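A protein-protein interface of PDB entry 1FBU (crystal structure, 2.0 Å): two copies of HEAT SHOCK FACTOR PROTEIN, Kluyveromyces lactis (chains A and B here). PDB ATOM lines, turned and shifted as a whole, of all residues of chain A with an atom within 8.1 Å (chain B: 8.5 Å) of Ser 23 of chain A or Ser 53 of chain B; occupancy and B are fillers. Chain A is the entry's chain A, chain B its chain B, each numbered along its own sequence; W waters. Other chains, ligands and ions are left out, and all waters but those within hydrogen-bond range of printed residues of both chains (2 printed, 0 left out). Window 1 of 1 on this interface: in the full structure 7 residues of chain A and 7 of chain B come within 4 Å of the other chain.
A ring nitrogen (NE2) of His 21 of chain A sits close to the guanidinium group of Arg 56 of chain B (3.4 Å).
The backbone carbonyl oxygen (O) of Trp 22 of chain A is in hydrogen-bond range of the guanidinium group (NH1) of Arg 56 of chain B, 3.4 Å away.
O of Ser 23 of chain A sits at hydrogen-bond distance from OG of Ser 53 of chain B, at 2.8 Å.
OG of Ser 53 of chain B lies within hydrogen-bond range of O of Thr 24 of chain A (3.3 Å).
The guanidinium group (NH1) of Arg 56 of chain B is in hydrogen-bond range of the side-chain hydroxyl (OG1) of Thr 24 of chain A, at 3.1 Å.
O of His 48 of chain B lies close to N of Glu 27 of chain A (3.3 Å).
O of His 48 of chain B sits close to O of Gly 26 of chain A (3.3 Å).
Of the printed residues of chain B, His 21 of chain A touches Arg 56 (3.4 Å).
Of the printed residues of chain B, Trp 22 of chain A touches Asn 50, Ala 52 and Arg 56.
Of the printed residues of chain B, Ser 23 of chain A touches Ser 53.
Printed residues of chain B within 4 Å of Thr 24 of chain A: Ser 53, Arg 56 and Gln 57.
Gly 26 of chain A touches two residues of chain B.
Of the printed residues of chain B, Glu 27 of chain A touches His 48 (3.1 Å), Ser 49 (3.9 Å) and Asn 50 (3.6 Å).
No residue of chain B comes within 4 Å of Ser 28 of chain A.
Ile 29 of chain A touches none of the printed residues of chain B.
Leu 42 of chain B touches none of the printed residues of chain A.
Of chain A, only Ser 23 (2.8 Å), Thr 24 (3.3 Å) and Gly 26 (3.9 Å) come within 4 Å of Ser 53 of chain B.
Printed residues of chain A within 4 Å of Gln 57 of chain B: Thr 24 (3.2 Å).
Of the 18 printed residues of chain A, 6 touch a printed residue of chain B.
Hydrophobic or aromatic side chains of chain A within 4 Å of the printed part of chain B: His 21 and Trp 22.
Of the 17 printed residues of chain B, 7 touch a printed residue of chain A.
Printed residues of chain B that touch a printed residue of chain A: His 48, Ser 49, Asn 50, Ala 52, Ser 53, Arg 56 and Gln 57.
Hydrophobic or aromatic side chains of chain B within 4 Å of the printed part of chain A: Ala 52.
Among the printed residues, no Asp or Glu carboxylate lies within 4 Å of a Lys or Arg side-chain nitrogen of the other chain.
The indole nitrogen (NE1) of Trp 22 of chain A lies within hydrogen-bond range of the side-chain amide oxygen (OD1) of Asn 12 of chain A (2.9 Å).
The backbone carbonyl oxygen of His 21 of chain A sits at hydrogen-bond distance from the backbone NH of Val 30 of chain A.
OG of Ser 23 of chain A lies close to O of Gly 26 of chain A (3.1 Å).
The backbone carbonyl oxygen (O) of Ser 28 of chain A sits at hydrogen-bond distance from the backbone NH (N) of Ser 23 of chain A, 2.8 Å away.
The side-chain amide oxygen (OD1) of Asn 50 of chain B is in hydrogen-bond range of the backbone NH (N) of Ala 52 of chain B, 3.1 Å away.
OD1 of Asn 50 of chain B sits at hydrogen-bond distance from N of Ser 53 of chain B (2.7 Å).
No position is printed for both chains.
Among the printed residues, merely in contact across the chains: Trp 22 of chain A with Asn 50 of chain B (3.5 Å), Trp 22 of chain A with Ala 52 of chain B (3.4 Å), Thr 24 of chain A with Gln 57 of chain B (3.2 Å), Gly 26 of chain A with Ser 53 of chain B (3.9 Å), Glu 27 of chain A with Ser 49 of chain B (3.9 Å) and Glu 27 of chain A with Asn 50 of chain B (3.6 Å).
Water W1 lies within hydrogen-bond range of OG of Ser 53 of chain B (2.8 Å), O of Ser 23 of chain A (3.0 Å) and NH1 of Arg 56 of chain B (3.1 Å).
Water W2 bridges the side-chain amide nitrogen of Asn 50 of chain B (3.3 Å) and the side-chain carboxylate of Glu 27 of chain A (3.4 Å).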
ATOM      1  N   VAL A  11      -4.122 -19.166 -33.937  1.00  0.00           N
ATOM      2  CA  VAL A  11      -2.987 -19.016 -33.035  1.00  0.00           C
ATOM      3  C   VAL A  11      -2.200 -17.717 -33.187  1.00  0.00           C
ATOM      4  O   VAL A  11      -1.766 -17.132 -32.192  1.00  0.00           O
ATOM      5  CB  VAL A  11      -2.005 -20.206 -33.190  1.00  0.00           C
ATOM      6  CG1 VAL A  11      -0.822 -20.044 -32.248  1.00  0.00           C
ATOM      7  CG2 VAL A  11      -2.734 -21.513 -32.901  1.00  0.00           C
ATOM      8  N   ASN A  12      -2.015 -17.259 -34.421  1.00  0.00           N
ATOM      9  CA  ASN A  12      -1.244 -16.038 -34.648  1.00  0.00           C
ATOM     10  C   ASN A  12      -2.029 -14.727 -34.705  1.00  0.00           C
ATOM     11  O   ASN A  12      -1.515 -13.703 -35.157  1.00  0.00           O
ATOM     12  CB  ASN A  12      -0.372 -16.205 -35.898  1.00  0.00           C
ATOM     13  CG  ASN A  12       0.730 -17.229 -35.691  1.00  0.00           C
ATOM     14  OD1 ASN A  12       1.250 -17.367 -34.584  1.00  0.00           O
ATOM     15  ND2 ASN A  12       1.102 -17.939 -36.752  1.00  0.00           N
ATOM     16  N   ILE A  20      -5.759 -19.268 -26.567  1.00  0.00           N
ATOM     17  CA  ILE A  20      -4.804 -20.151 -27.219  1.00  0.00           C
ATOM     18  C   ILE A  20      -3.637 -19.283 -27.662  1.00  0.00           C
ATOM     19  O   ILE A  20      -3.832 -18.222 -28.251  1.00  0.00           O
ATOM     20  CB  ILE A  20      -5.457 -20.889 -28.427  1.00  0.00           C
ATOM     21  CG1 ILE A  20      -4.442 -21.833 -29.076  1.00  0.00           C
ATOM     22  CG2 ILE A  20      -6.012 -19.881 -29.431  1.00  0.00           C
ATOM     23  CD1 ILE A  20      -5.067 -22.798 -30.084  1.00  0.00           C
ATOM     24  N   HIS A  21      -2.422 -19.718 -27.347  1.00  0.00           N
ATOM     25  CA  HIS A  21      -1.245 -18.933 -27.706  1.00  0.00           C
ATOM     26  C   HIS A  21       0.039 -19.744 -27.655  1.00  0.00           C
ATOM     27  O   HIS A  21       0.082 -20.829 -27.071  1.00  0.00           O
ATOM     28  CB  HIS A  21      -1.097 -17.730 -26.760  1.00  0.00           C
ATOM     29  CG  HIS A  21      -0.871 -18.104 -25.323  1.00  0.00           C
ATOM     30  ND1 HIS A  21      -1.866 -18.042 -24.372  1.00  0.00           N
ATOM     31  CD2 HIS A  21       0.229 -18.570 -24.683  1.00  0.00           C
ATOM     32  CE1 HIS A  21      -1.389 -18.455 -23.209  1.00  0.00           C
ATOM     33  NE2 HIS A  21      -0.120 -18.781 -23.371  1.00  0.00           N
ATOM     34  N   TRP A  22       1.088 -19.207 -28.274  1.00  0.00           N
ATOM     35  CA  TRP A  22       2.391 -19.861 -28.256  1.00  0.00           C
ATOM     36  C   TRP A  22       2.881 -19.773 -26.815  1.00  0.00           C
ATOM     37  O   TRP A  22       2.646 -18.774 -26.151  1.00  0.00           O
ATOM     38  CB  TRP A  22       3.373 -19.127 -29.173  1.00  0.00           C
ATOM     39  CG  TRP A  22       3.151 -19.388 -30.616  1.00  0.00           C
ATOM     40  CD1 TRP A  22       2.570 -18.552 -31.524  1.00  0.00           C
ATOM     41  CD2 TRP A  22       3.529 -20.565 -31.335  1.00  0.00           C
ATOM     42  NE1 TRP A  22       2.566 -19.132 -32.769  1.00  0.00           N
ATOM     43  CE2 TRP A  22       3.152 -20.369 -32.683  1.00  0.00           C
ATOM     44  CE3 TRP A  22       4.152 -21.768 -30.972  1.00  0.00           C
ATOM     45  CZ2 TRP A  22       3.380 -21.326 -33.669  1.00  0.00           C
ATOM     46  CZ3 TRP A  22       4.379 -22.726 -31.955  1.00  0.00           C
ATOM     47  CH2 TRP A  22       3.994 -22.495 -33.292  1.00  0.00           C
ATOM     48  N   SER A  23       3.557 -20.807 -26.329  1.00  0.00           N
ATOM     49  CA  SER A  23       4.034 -20.799 -24.949  1.00  0.00           C
ATOM     50  C   SER A  23       5.147 -19.787 -24.713  1.00  0.00           C
ATOM     51  O   SER A  23       5.943 -19.501 -25.605  1.00  0.00           O
ATOM     52  CB  SER A  23       4.515 -22.194 -24.537  1.00  0.00           C
ATOM     53  OG  SER A  23       5.640 -22.601 -25.291  1.00  0.00           O
ATOM     54  N   THR A  24       5.189 -19.250 -23.497  1.00  0.00           N
ATOM     55  CA  THR A  24       6.198 -18.272 -23.120  1.00  0.00           C
ATOM     56  C   THR A  24       7.565 -18.941 -23.120  1.00  0.00           C
ATOM     57  O   THR A  24       8.487 -18.497 -23.806  1.00  0.00           O
ATOM     58  CB  THR A  24       5.914 -17.702 -21.718  1.00  0.00           C
ATOM     59  OG1 THR A  24       4.604 -17.119 -21.696  1.00  0.00           O
ATOM     60  CG2 THR A  24       6.944 -16.641 -21.357  1.00  0.00           C
ATOM     61  N   SER A  25       7.688 -20.017 -22.349  1.00  0.00           N
ATOM     62  CA  SER A  25       8.942 -20.755 -22.268  1.00  0.00           C
ATOM     63  C   SER A  25       8.806 -22.100 -22.968  1.00  0.00           C
ATOM     64  O   SER A  25       8.452 -23.104 -22.347  1.00  0.00           O
ATOM     65  CB  SER A  25       9.347 -20.964 -20.804  1.00  0.00           C
ATOM     66  OG  SER A  25       8.351 -21.669 -20.085  1.00  0.00           O
ATOM     67  N   GLY A  26       9.082 -22.112 -24.266  1.00  0.00           N
ATOM     68  CA  GLY A  26       8.983 -23.342 -25.032  1.00  0.00           C
ATOM     69  C   GLY A  26       8.501 -23.080 -26.443  1.00  0.00           C
ATOM     70  O   GLY A  26       8.289 -21.929 -26.831  1.00  0.00           O
ATOM     71  N   GLU A  27       8.332 -24.153 -27.211  1.00  0.00           N
ATOM     72  CA  GLU A  27       7.874 -24.054 -28.591  1.00  0.00           C
ATOM     73  C   GLU A  27       6.571 -24.826 -28.743  1.00  0.00           C
ATOM     74  O   GLU A  27       6.407 -25.595 -29.689  1.00  0.00           O
ATOM     75  CB  GLU A  27       8.907 -24.663 -29.534  1.00  0.00           C
ATOM     76  CG  GLU A  27      10.294 -24.080 -29.417  1.00  0.00           C
ATOM     77  CD  GLU A  27      11.347 -25.026 -29.950  1.00  0.00           C
ATOM     78  OE1 GLU A  27      11.581 -26.075 -29.308  1.00  0.00           O
ATOM     79  OE2 GLU A  27      11.934 -24.727 -31.011  1.00  0.00           O
ATOM     80  N   SER A  28       5.648 -24.633 -27.813  1.00  0.00           N
ATOM     81  CA  SER A  28       4.384 -25.346 -27.876  1.00  0.00           C
ATOM     82  C   SER A  28       3.208 -24.389 -27.972  1.00  0.00           C
ATOM     83  O   SER A  28       3.357 -23.178 -27.793  1.00  0.00           O
ATOM     84  CB  SER A  28       4.230 -26.232 -26.640  1.00  0.00           C
ATOM     85  OG  SER A  28       4.213 -25.455 -25.453  1.00  0.00           O
ATOM     86  N   ILE A  29       2.040 -24.944 -28.275  1.00  0.00           N
ATOM     87  CA  ILE A  29       0.818 -24.167 -28.370  1.00  0.00           C
ATOM     88  C   ILE A  29       0.055 -24.476 -27.092  1.00  0.00           C
ATOM     89  O   ILE A  29      -0.105 -25.637 -26.728  1.00  0.00           O
ATOM     90  CB  ILE A  29      -0.021 -24.584 -29.591  1.00  0.00           C
ATOM     91  CG1 ILE A  29       0.669 -24.116 -30.877  1.00  0.00           C
ATOM     92  CG2 ILE A  29      -1.422 -23.992 -29.489  1.00  0.00           C
ATOM     93  CD1 ILE A  29      -0.002 -24.616 -32.148  1.00  0.00           C
ATOM     94  N   VAL A  30      -0.413 -23.438 -26.411  1.00  0.00           N
ATOM     95  CA  VAL A  30      -1.119 -23.643 -25.161  1.00  0.00           C
ATOM     96  C   VAL A  30      -2.571 -23.211 -25.196  1.00  0.00           C
ATOM     97  O   VAL A  30      -2.897 -22.134 -25.688  1.00  0.00           O
ATOM     98  CB  VAL A  30      -0.438 -22.874 -23.992  1.00  0.00           C
ATOM     99  CG1 VAL A  30      -1.168 -23.165 -22.687  1.00  0.00           C
ATOM    100  CG2 VAL A  30       1.032 -23.264 -23.883  1.00  0.00           C
ATOM    101  N   VAL A  31      -3.432 -24.083 -24.680  1.00  0.00           N
ATOM    102  CA  VAL A  31      -4.855 -23.802 -24.545  1.00  0.00           C
ATOM    103  C   VAL A  31      -4.993 -23.805 -23.021  1.00  0.00           C
ATOM    104  O   VAL A  31      -5.100 -24.867 -22.401  1.00  0.00           O
ATOM    105  CB  VAL A  31      -5.734 -24.925 -25.148  1.00  0.00           C
ATOM    106  CG1 VAL A  31      -7.196 -24.678 -24.812  1.00  0.00           C
ATOM    107  CG2 VAL A  31      -5.560 -24.973 -26.654  1.00  0.00           C
ATOM    108  N   ARG A  81      -6.159 -27.724 -18.946  1.00  0.00           N
ATOM    109  CA  ARG A  81      -5.023 -27.064 -19.586  1.00  0.00           C
ATOM    110  C   ARG A  81      -4.374 -28.044 -20.548  1.00  0.00           C
ATOM    111  O   ARG A  81      -3.948 -29.131 -20.149  1.00  0.00           O
ATOM    112  CB  ARG A  81      -3.979 -26.597 -18.561  1.00  0.00           C
ATOM    113  CG  ARG A  81      -2.815 -25.843 -19.202  1.00  0.00           C
ATOM    114  CD  ARG A  81      -1.712 -25.523 -18.197  1.00  0.00           C
ATOM    115  NE  ARG A  81      -0.579 -24.831 -18.818  1.00  0.00           N
ATOM    116  CZ  ARG A  81      -0.497 -23.514 -19.003  1.00  0.00           C
ATOM    117  NH1 ARG A  81      -1.482 -22.714 -18.612  1.00  0.00           N
ATOM    118  NH2 ARG A  81       0.581 -22.994 -19.579  1.00  0.00           N
ATOM    119  N   GLU A  83      -1.439 -28.501 -23.671  1.00  0.00           N
ATOM    120  CA  GLU A  83      -0.272 -27.953 -24.344  1.00  0.00           C
ATOM    121  C   GLU A  83       0.091 -28.947 -25.428  1.00  0.00           C
ATOM    122  O   GLU A  83       0.087 -30.161 -25.187  1.00  0.00           O
ATOM    123  CB  GLU A  83       0.889 -27.788 -23.365  1.00  0.00           C
ATOM    124  CG  GLU A  83       2.018 -26.922 -23.895  1.00  0.00           C
ATOM    125  CD  GLU A  83       3.025 -26.558 -22.815  1.00  0.00           C
ATOM    126  OE1 GLU A  83       2.609 -26.454 -21.639  1.00  0.00           O
ATOM    127  OE2 GLU A  83       4.220 -26.365 -23.142  1.00  0.00           O
ATOM    128  N   PHE A  84       0.386 -28.433 -26.619  1.00  0.00           N
ATOM    129  CA  PHE A  84       0.726 -29.276 -27.762  1.00  0.00           C
ATOM    130  C   PHE A  84       2.103 -28.964 -28.335  1.00  0.00           C
ATOM    131  O   PHE A  84       2.486 -27.800 -28.467  1.00  0.00           O
ATOM    132  CB  PHE A  84      -0.298 -29.083 -28.877  1.00  0.00           C
ATOM    133  CG  PHE A  84      -1.714 -29.363 -28.467  1.00  0.00           C
ATOM    134  CD1 PHE A  84      -2.228 -30.655 -28.528  1.00  0.00           C
ATOM    135  CD2 PHE A  84      -2.543 -28.330 -28.050  1.00  0.00           C
ATOM    136  CE1 PHE A  84      -3.556 -30.913 -28.180  1.00  0.00           C
ATOM    137  CE2 PHE A  84      -3.872 -28.578 -27.699  1.00  0.00           C
ATOM    138  CZ  PHE A  84      -4.373 -29.872 -27.767  1.00  0.00           C
ATOM    139  N   GLU A  85       2.835 -30.015 -28.682  1.00  0.00           N
ATOM    140  CA  GLU A  85       4.151 -29.865 -29.284  1.00  0.00           C
ATOM    141  C   GLU A  85       4.123 -30.561 -30.632  1.00  0.00           C
ATOM    142  O   GLU A  85       3.325 -31.470 -30.855  1.00  0.00           O
ATOM    143  CB  GLU A  85       5.233 -30.508 -28.423  1.00  0.00           C
ATOM    144  CG  GLU A  85       5.485 -29.818 -27.114  1.00  0.00           C
ATOM    145  CD  GLU A  85       6.683 -30.392 -26.399  1.00  0.00           C
ATOM    146  OE1 GLU A  85       6.782 -31.638 -26.317  1.00  0.00           O
ATOM    147  OE2 GLU A  85       7.520 -29.601 -25.917  1.00  0.00           O
ATOM    148  N   PHE B   3      12.454 -11.222 -19.299  1.00  0.00           N
ATOM    149  CA  PHE B   3      12.518 -11.073 -20.745  1.00  0.00           C
ATOM    150  C   PHE B   3      13.243  -9.796 -21.145  1.00  0.00           C
ATOM    151  O   PHE B   3      14.164  -9.829 -21.956  1.00  0.00           O
ATOM    152  CB  PHE B   3      11.119 -11.050 -21.356  1.00  0.00           C
ATOM    153  CG  PHE B   3      11.123 -10.893 -22.850  1.00  0.00           C
ATOM    154  CD1 PHE B   3      11.471 -11.960 -23.673  1.00  0.00           C
ATOM    155  CD2 PHE B   3      10.821  -9.664 -23.435  1.00  0.00           C
ATOM    156  CE1 PHE B   3      11.523 -11.807 -25.059  1.00  0.00           C
ATOM    157  CE2 PHE B   3      10.870  -9.500 -24.817  1.00  0.00           C
ATOM    158  CZ  PHE B   3      11.223 -10.575 -25.632  1.00  0.00           C
ATOM    159  N   LEU B  42      18.760 -16.295 -31.063  1.00  0.00           N
ATOM    160  CA  LEU B  42      17.693 -16.721 -30.176  1.00  0.00           C
ATOM    161  C   LEU B  42      18.084 -17.809 -29.177  1.00  0.00           C
ATOM    162  O   LEU B  42      17.806 -17.687 -27.990  1.00  0.00           O
ATOM    163  CB  LEU B  42      16.478 -17.163 -31.001  1.00  0.00           C
ATOM    164  CG  LEU B  42      15.117 -17.104 -30.306  1.00  0.00           C
ATOM    165  CD1 LEU B  42      14.874 -15.708 -29.734  1.00  0.00           C
ATOM    166  CD2 LEU B  42      14.028 -17.456 -31.311  1.00  0.00           C
ATOM    167  N   PHE B  46      17.348 -17.450 -25.377  1.00  0.00           N
ATOM    168  CA  PHE B  46      16.096 -18.155 -25.135  1.00  0.00           C
ATOM    169  C   PHE B  46      16.182 -19.586 -25.641  1.00  0.00           C
ATOM    170  O   PHE B  46      16.038 -19.846 -26.838  1.00  0.00           O
ATOM    171  CB  PHE B  46      14.948 -17.431 -25.841  1.00  0.00           C
ATOM    172  CG  PHE B  46      14.764 -16.015 -25.394  1.00  0.00           C
ATOM    173  CD1 PHE B  46      14.199 -15.733 -24.154  1.00  0.00           C
ATOM    174  CD2 PHE B  46      15.182 -14.959 -26.196  1.00  0.00           C
ATOM    175  CE1 PHE B  46      14.056 -14.420 -23.721  1.00  0.00           C
ATOM    176  CE2 PHE B  46      15.045 -13.643 -25.773  1.00  0.00           C
ATOM    177  CZ  PHE B  46      14.481 -13.372 -24.534  1.00  0.00           C
ATOM    178  N   LYS B  47      16.421 -20.513 -24.722  1.00  0.00           N
ATOM    179  CA  LYS B  47      16.522 -21.924 -25.068  1.00  0.00           C
ATOM    180  C   LYS B  47      15.122 -22.462 -25.338  1.00  0.00           C
ATOM    181  O   LYS B  47      14.181 -22.136 -24.616  1.00  0.00           O
ATOM    182  CB  LYS B  47      17.143 -22.700 -23.906  1.00  0.00           C
ATOM    183  CG  LYS B  47      18.195 -21.920 -23.126  1.00  0.00           C
ATOM    184  CD  LYS B  47      19.400 -21.574 -23.982  1.00  0.00           C
ATOM    185  CE  LYS B  47      20.409 -20.754 -23.197  1.00  0.00           C
ATOM    186  NZ  LYS B  47      21.589 -20.390 -24.029  1.00  0.00           N
ATOM    187  N   HIS B  48      14.983 -23.277 -26.378  1.00  0.00           N
ATOM    188  CA  HIS B  48      13.691 -23.868 -26.719  1.00  0.00           C
ATOM    189  C   HIS B  48      12.601 -22.853 -27.066  1.00  0.00           C
ATOM    190  O   HIS B  48      11.427 -23.060 -26.757  1.00  0.00           O
ATOM    191  CB  HIS B  48      13.209 -24.749 -25.564  1.00  0.00           C
ATOM    192  CG  HIS B  48      14.155 -25.857 -25.224  1.00  0.00           C
ATOM    193  ND1 HIS B  48      14.465 -26.198 -23.926  1.00  0.00           N
ATOM    194  CD2 HIS B  48      14.856 -26.703 -26.014  1.00  0.00           C
ATOM    195  CE1 HIS B  48      15.319 -27.205 -23.930  1.00  0.00           C
ATOM    196  NE2 HIS B  48      15.573 -27.531 -25.185  1.00  0.00           N
ATOM    197  N   SER B  49      12.984 -21.761 -27.710  1.00  0.00           N
ATOM    198  CA  SER B  49      12.017 -20.743 -28.098  1.00  0.00           C
ATOM    199  C   SER B  49      12.029 -20.606 -29.618  1.00  0.00           C
ATOM    200  O   SER B  49      13.016 -20.951 -30.267  1.00  0.00           O
ATOM    201  CB  SER B  49      12.381 -19.407 -27.443  1.00  0.00           C
ATOM    202  OG  SER B  49      11.421 -18.407 -27.730  1.00  0.00           O
ATOM    203  N   ASN B  50      10.922 -20.139 -30.188  1.00  0.00           N
ATOM    204  CA  ASN B  50      10.849 -19.938 -31.632  1.00  0.00           C
ATOM    205  C   ASN B  50      10.555 -18.465 -31.883  1.00  0.00           C
ATOM    206  O   ASN B  50      10.360 -17.704 -30.938  1.00  0.00           O
ATOM    207  CB  ASN B  50       9.773 -20.826 -32.276  1.00  0.00           C
ATOM    208  CG  ASN B  50       8.402 -20.629 -31.670  1.00  0.00           C
ATOM    209  OD1 ASN B  50       7.936 -19.506 -31.504  1.00  0.00           O
ATOM    210  ND2 ASN B  50       7.733 -21.735 -31.351  1.00  0.00           N
ATOM    211  N   PHE B  51      10.511 -18.062 -33.147  1.00  0.00           N
ATOM    212  CA  PHE B  51      10.281 -16.658 -33.469  1.00  0.00           C
ATOM    213  C   PHE B  51       8.932 -16.124 -33.005  1.00  0.00           C
ATOM    214  O   PHE B  51       8.846 -15.011 -32.494  1.00  0.00           O
ATOM    215  CB  PHE B  51      10.430 -16.424 -34.973  1.00  0.00           C
ATOM    216  CG  PHE B  51      10.559 -14.973 -35.346  1.00  0.00           C
ATOM    217  CD1 PHE B  51      11.646 -14.224 -34.901  1.00  0.00           C
ATOM    218  CD2 PHE B  51       9.596 -14.354 -36.139  1.00  0.00           C
ATOM    219  CE1 PHE B  51      11.773 -12.874 -35.244  1.00  0.00           C
ATOM    220  CE2 PHE B  51       9.711 -13.009 -36.488  1.00  0.00           C
ATOM    221  CZ  PHE B  51      10.803 -12.267 -36.039  1.00  0.00           C
ATOM    222  N   ALA B  52       7.877 -16.911 -33.194  1.00  0.00           N
ATOM    223  CA  ALA B  52       6.544 -16.488 -32.790  1.00  0.00           C
ATOM    224  C   ALA B  52       6.476 -16.229 -31.292  1.00  0.00           C
ATOM    225  O   ALA B  52       5.847 -15.265 -30.851  1.00  0.00           O
ATOM    226  CB  ALA B  52       5.515 -17.547 -33.182  1.00  0.00           C
ATOM    227  N   SER B  53       7.112 -17.095 -30.509  1.00  0.00           N
ATOM    228  CA  SER B  53       7.116 -16.947 -29.059  1.00  0.00           C
ATOM    229  C   SER B  53       7.851 -15.673 -28.656  1.00  0.00           C
ATOM    230  O   SER B  53       7.432 -14.961 -27.740  1.00  0.00           O
ATOM    231  CB  SER B  53       7.778 -18.164 -28.410  1.00  0.00           C
ATOM    232  OG  SER B  53       7.829 -18.012 -27.003  1.00  0.00           O
ATOM    233  N   PHE B  54       8.952 -15.393 -29.346  1.00  0.00           N
ATOM    234  CA  PHE B  54       9.759 -14.203 -29.089  1.00  0.00           C
ATOM    235  C   PHE B  54       8.952 -12.944 -29.408  1.00  0.00           C
ATOM    236  O   PHE B  54       8.921 -11.992 -28.620  1.00  0.00           O
ATOM    237  CB  PHE B  54      11.024 -14.244 -29.954  1.00  0.00           C
ATOM    238  CG  PHE B  54      11.870 -13.006 -29.855  1.00  0.00           C
ATOM    239  CD1 PHE B  54      12.542 -12.697 -28.677  1.00  0.00           C
ATOM    240  CD2 PHE B  54      11.988 -12.146 -30.940  1.00  0.00           C
ATOM    241  CE1 PHE B  54      13.323 -11.547 -28.583  1.00  0.00           C
ATOM    242  CE2 PHE B  54      12.765 -10.997 -30.854  1.00  0.00           C
ATOM    243  CZ  PHE B  54      13.432 -10.696 -29.676  1.00  0.00           C
ATOM    244  N   VAL B  55       8.301 -12.941 -30.567  1.00  0.00           N
ATOM    245  CA  VAL B  55       7.491 -11.796 -30.967  1.00  0.00           C
ATOM    246  C   VAL B  55       6.324 -11.606 -29.999  1.00  0.00           C
ATOM    247  O   VAL B  55       5.942 -10.479 -29.699  1.00  0.00           O
ATOM    248  CB  VAL B  55       6.965 -11.962 -32.411  1.00  0.00           C
ATOM    249  CG1 VAL B  55       6.015 -10.818 -32.765  1.00  0.00           C
ATOM    250  CG2 VAL B  55       8.145 -11.970 -33.380  1.00  0.00           C
ATOM    251  N   ARG B  56       5.761 -12.706 -29.502  1.00  0.00           N
ATOM    252  CA  ARG B  56       4.662 -12.598 -28.553  1.00  0.00           C
ATOM    253  C   ARG B  56       5.133 -11.866 -27.293  1.00  0.00           C
ATOM    254  O   ARG B  56       4.397 -11.056 -26.733  1.00  0.00           O
ATOM    255  CB  ARG B  56       4.102 -13.989 -28.196  1.00  0.00           C
ATOM    256  CG  ARG B  56       3.126 -13.982 -27.011  1.00  0.00           C
ATOM    257  CD  ARG B  56       2.349 -15.301 -26.883  1.00  0.00           C
ATOM    258  NE  ARG B  56       1.513 -15.316 -25.683  1.00  0.00           N
ATOM    259  CZ  ARG B  56       1.945 -15.620 -24.463  1.00  0.00           C
ATOM    260  NH1 ARG B  56       3.213 -15.951 -24.256  1.00  0.00           N
ATOM    261  NH2 ARG B  56       1.104 -15.575 -23.438  1.00  0.00           N
ATOM    262  N   GLN B  57       6.361 -12.137 -26.858  1.00  0.00           N
ATOM    263  CA  GLN B  57       6.913 -11.488 -25.671  1.00  0.00           C
ATOM    264  C   GLN B  57       7.188 -10.018 -25.970  1.00  0.00           C
ATOM    265  O   GLN B  57       6.891  -9.147 -25.153  1.00  0.00           O
ATOM    266  CB  GLN B  57       8.201 -12.186 -25.239  1.00  0.00           C
ATOM    267  CG  GLN B  57       8.004 -13.655 -24.920  1.00  0.00           C
ATOM    268  CD  GLN B  57       8.084 -13.950 -23.450  1.00  0.00           C
ATOM    269  OE1 GLN B  57       9.137 -14.346 -22.936  1.00  0.00           O
ATOM    270  NE2 GLN B  57       6.973 -13.751 -22.752  1.00  0.00           N
ATOM    271  N   LEU B  58       7.755  -9.740 -27.141  1.00  0.00           N
ATOM    272  CA  LEU B  58       8.029  -8.359 -27.530  1.00  0.00           C
ATOM    273  C   LEU B  58       6.736  -7.555 -27.493  1.00  0.00           C
ATOM    274  O   LEU B  58       6.710  -6.430 -26.998  1.00  0.00           O
ATOM    275  CB  LEU B  58       8.610  -8.291 -28.945  1.00  0.00           C
ATOM    276  CG  LEU B  58      10.078  -8.659 -29.152  1.00  0.00           C
ATOM    277  CD1 LEU B  58      10.398  -8.609 -30.643  1.00  0.00           C
ATOM    278  CD2 LEU B  58      10.966  -7.678 -28.388  1.00  0.00           C
ATOM    279  N   ASN B  59       5.662  -8.137 -28.022  1.00  0.00           N
ATOM    280  CA  ASN B  59       4.372  -7.458 -28.048  1.00  0.00           C
ATOM    281  C   ASN B  59       3.871  -7.157 -26.641  1.00  0.00           C
ATOM    282  O   ASN B  59       3.240  -6.126 -26.406  1.00  0.00           O
ATOM    283  CB  ASN B  59       3.334  -8.301 -28.796  1.00  0.00           C
ATOM    284  CG  ASN B  59       3.606  -8.382 -30.292  1.00  0.00           C
ATOM    285  OD1 ASN B  59       2.883  -9.059 -31.024  1.00  0.00           O
ATOM    286  ND2 ASN B  59       4.649  -7.692 -30.754  1.00  0.00           N
ATOM    287  N   MET B  60       4.152  -8.054 -25.702  1.00  0.00           N
ATOM    288  CA  MET B  60       3.723  -7.858 -24.321  1.00  0.00           C
ATOM    289  C   MET B  60       4.394  -6.639 -23.699  1.00  0.00           C
ATOM    290  O   MET B  60       3.847  -6.018 -22.786  1.00  0.00           O
ATOM    291  CB  MET B  60       4.054  -9.088 -23.477  1.00  0.00           C
ATOM    292  CG  MET B  60       3.173 -10.288 -23.740  1.00  0.00           C
ATOM    293  SD  MET B  60       3.456 -11.574 -22.510  1.00  0.00           S
ATOM    294  CE  MET B  60       4.182 -12.861 -23.518  1.00  0.00           C
HETATM  295  O   HOH W   1       5.625 -16.571 -26.065  1.00  0.00           O
HETATM  296  O   HOH W   2       9.164 -24.242 -32.944  1.00  0.00           O
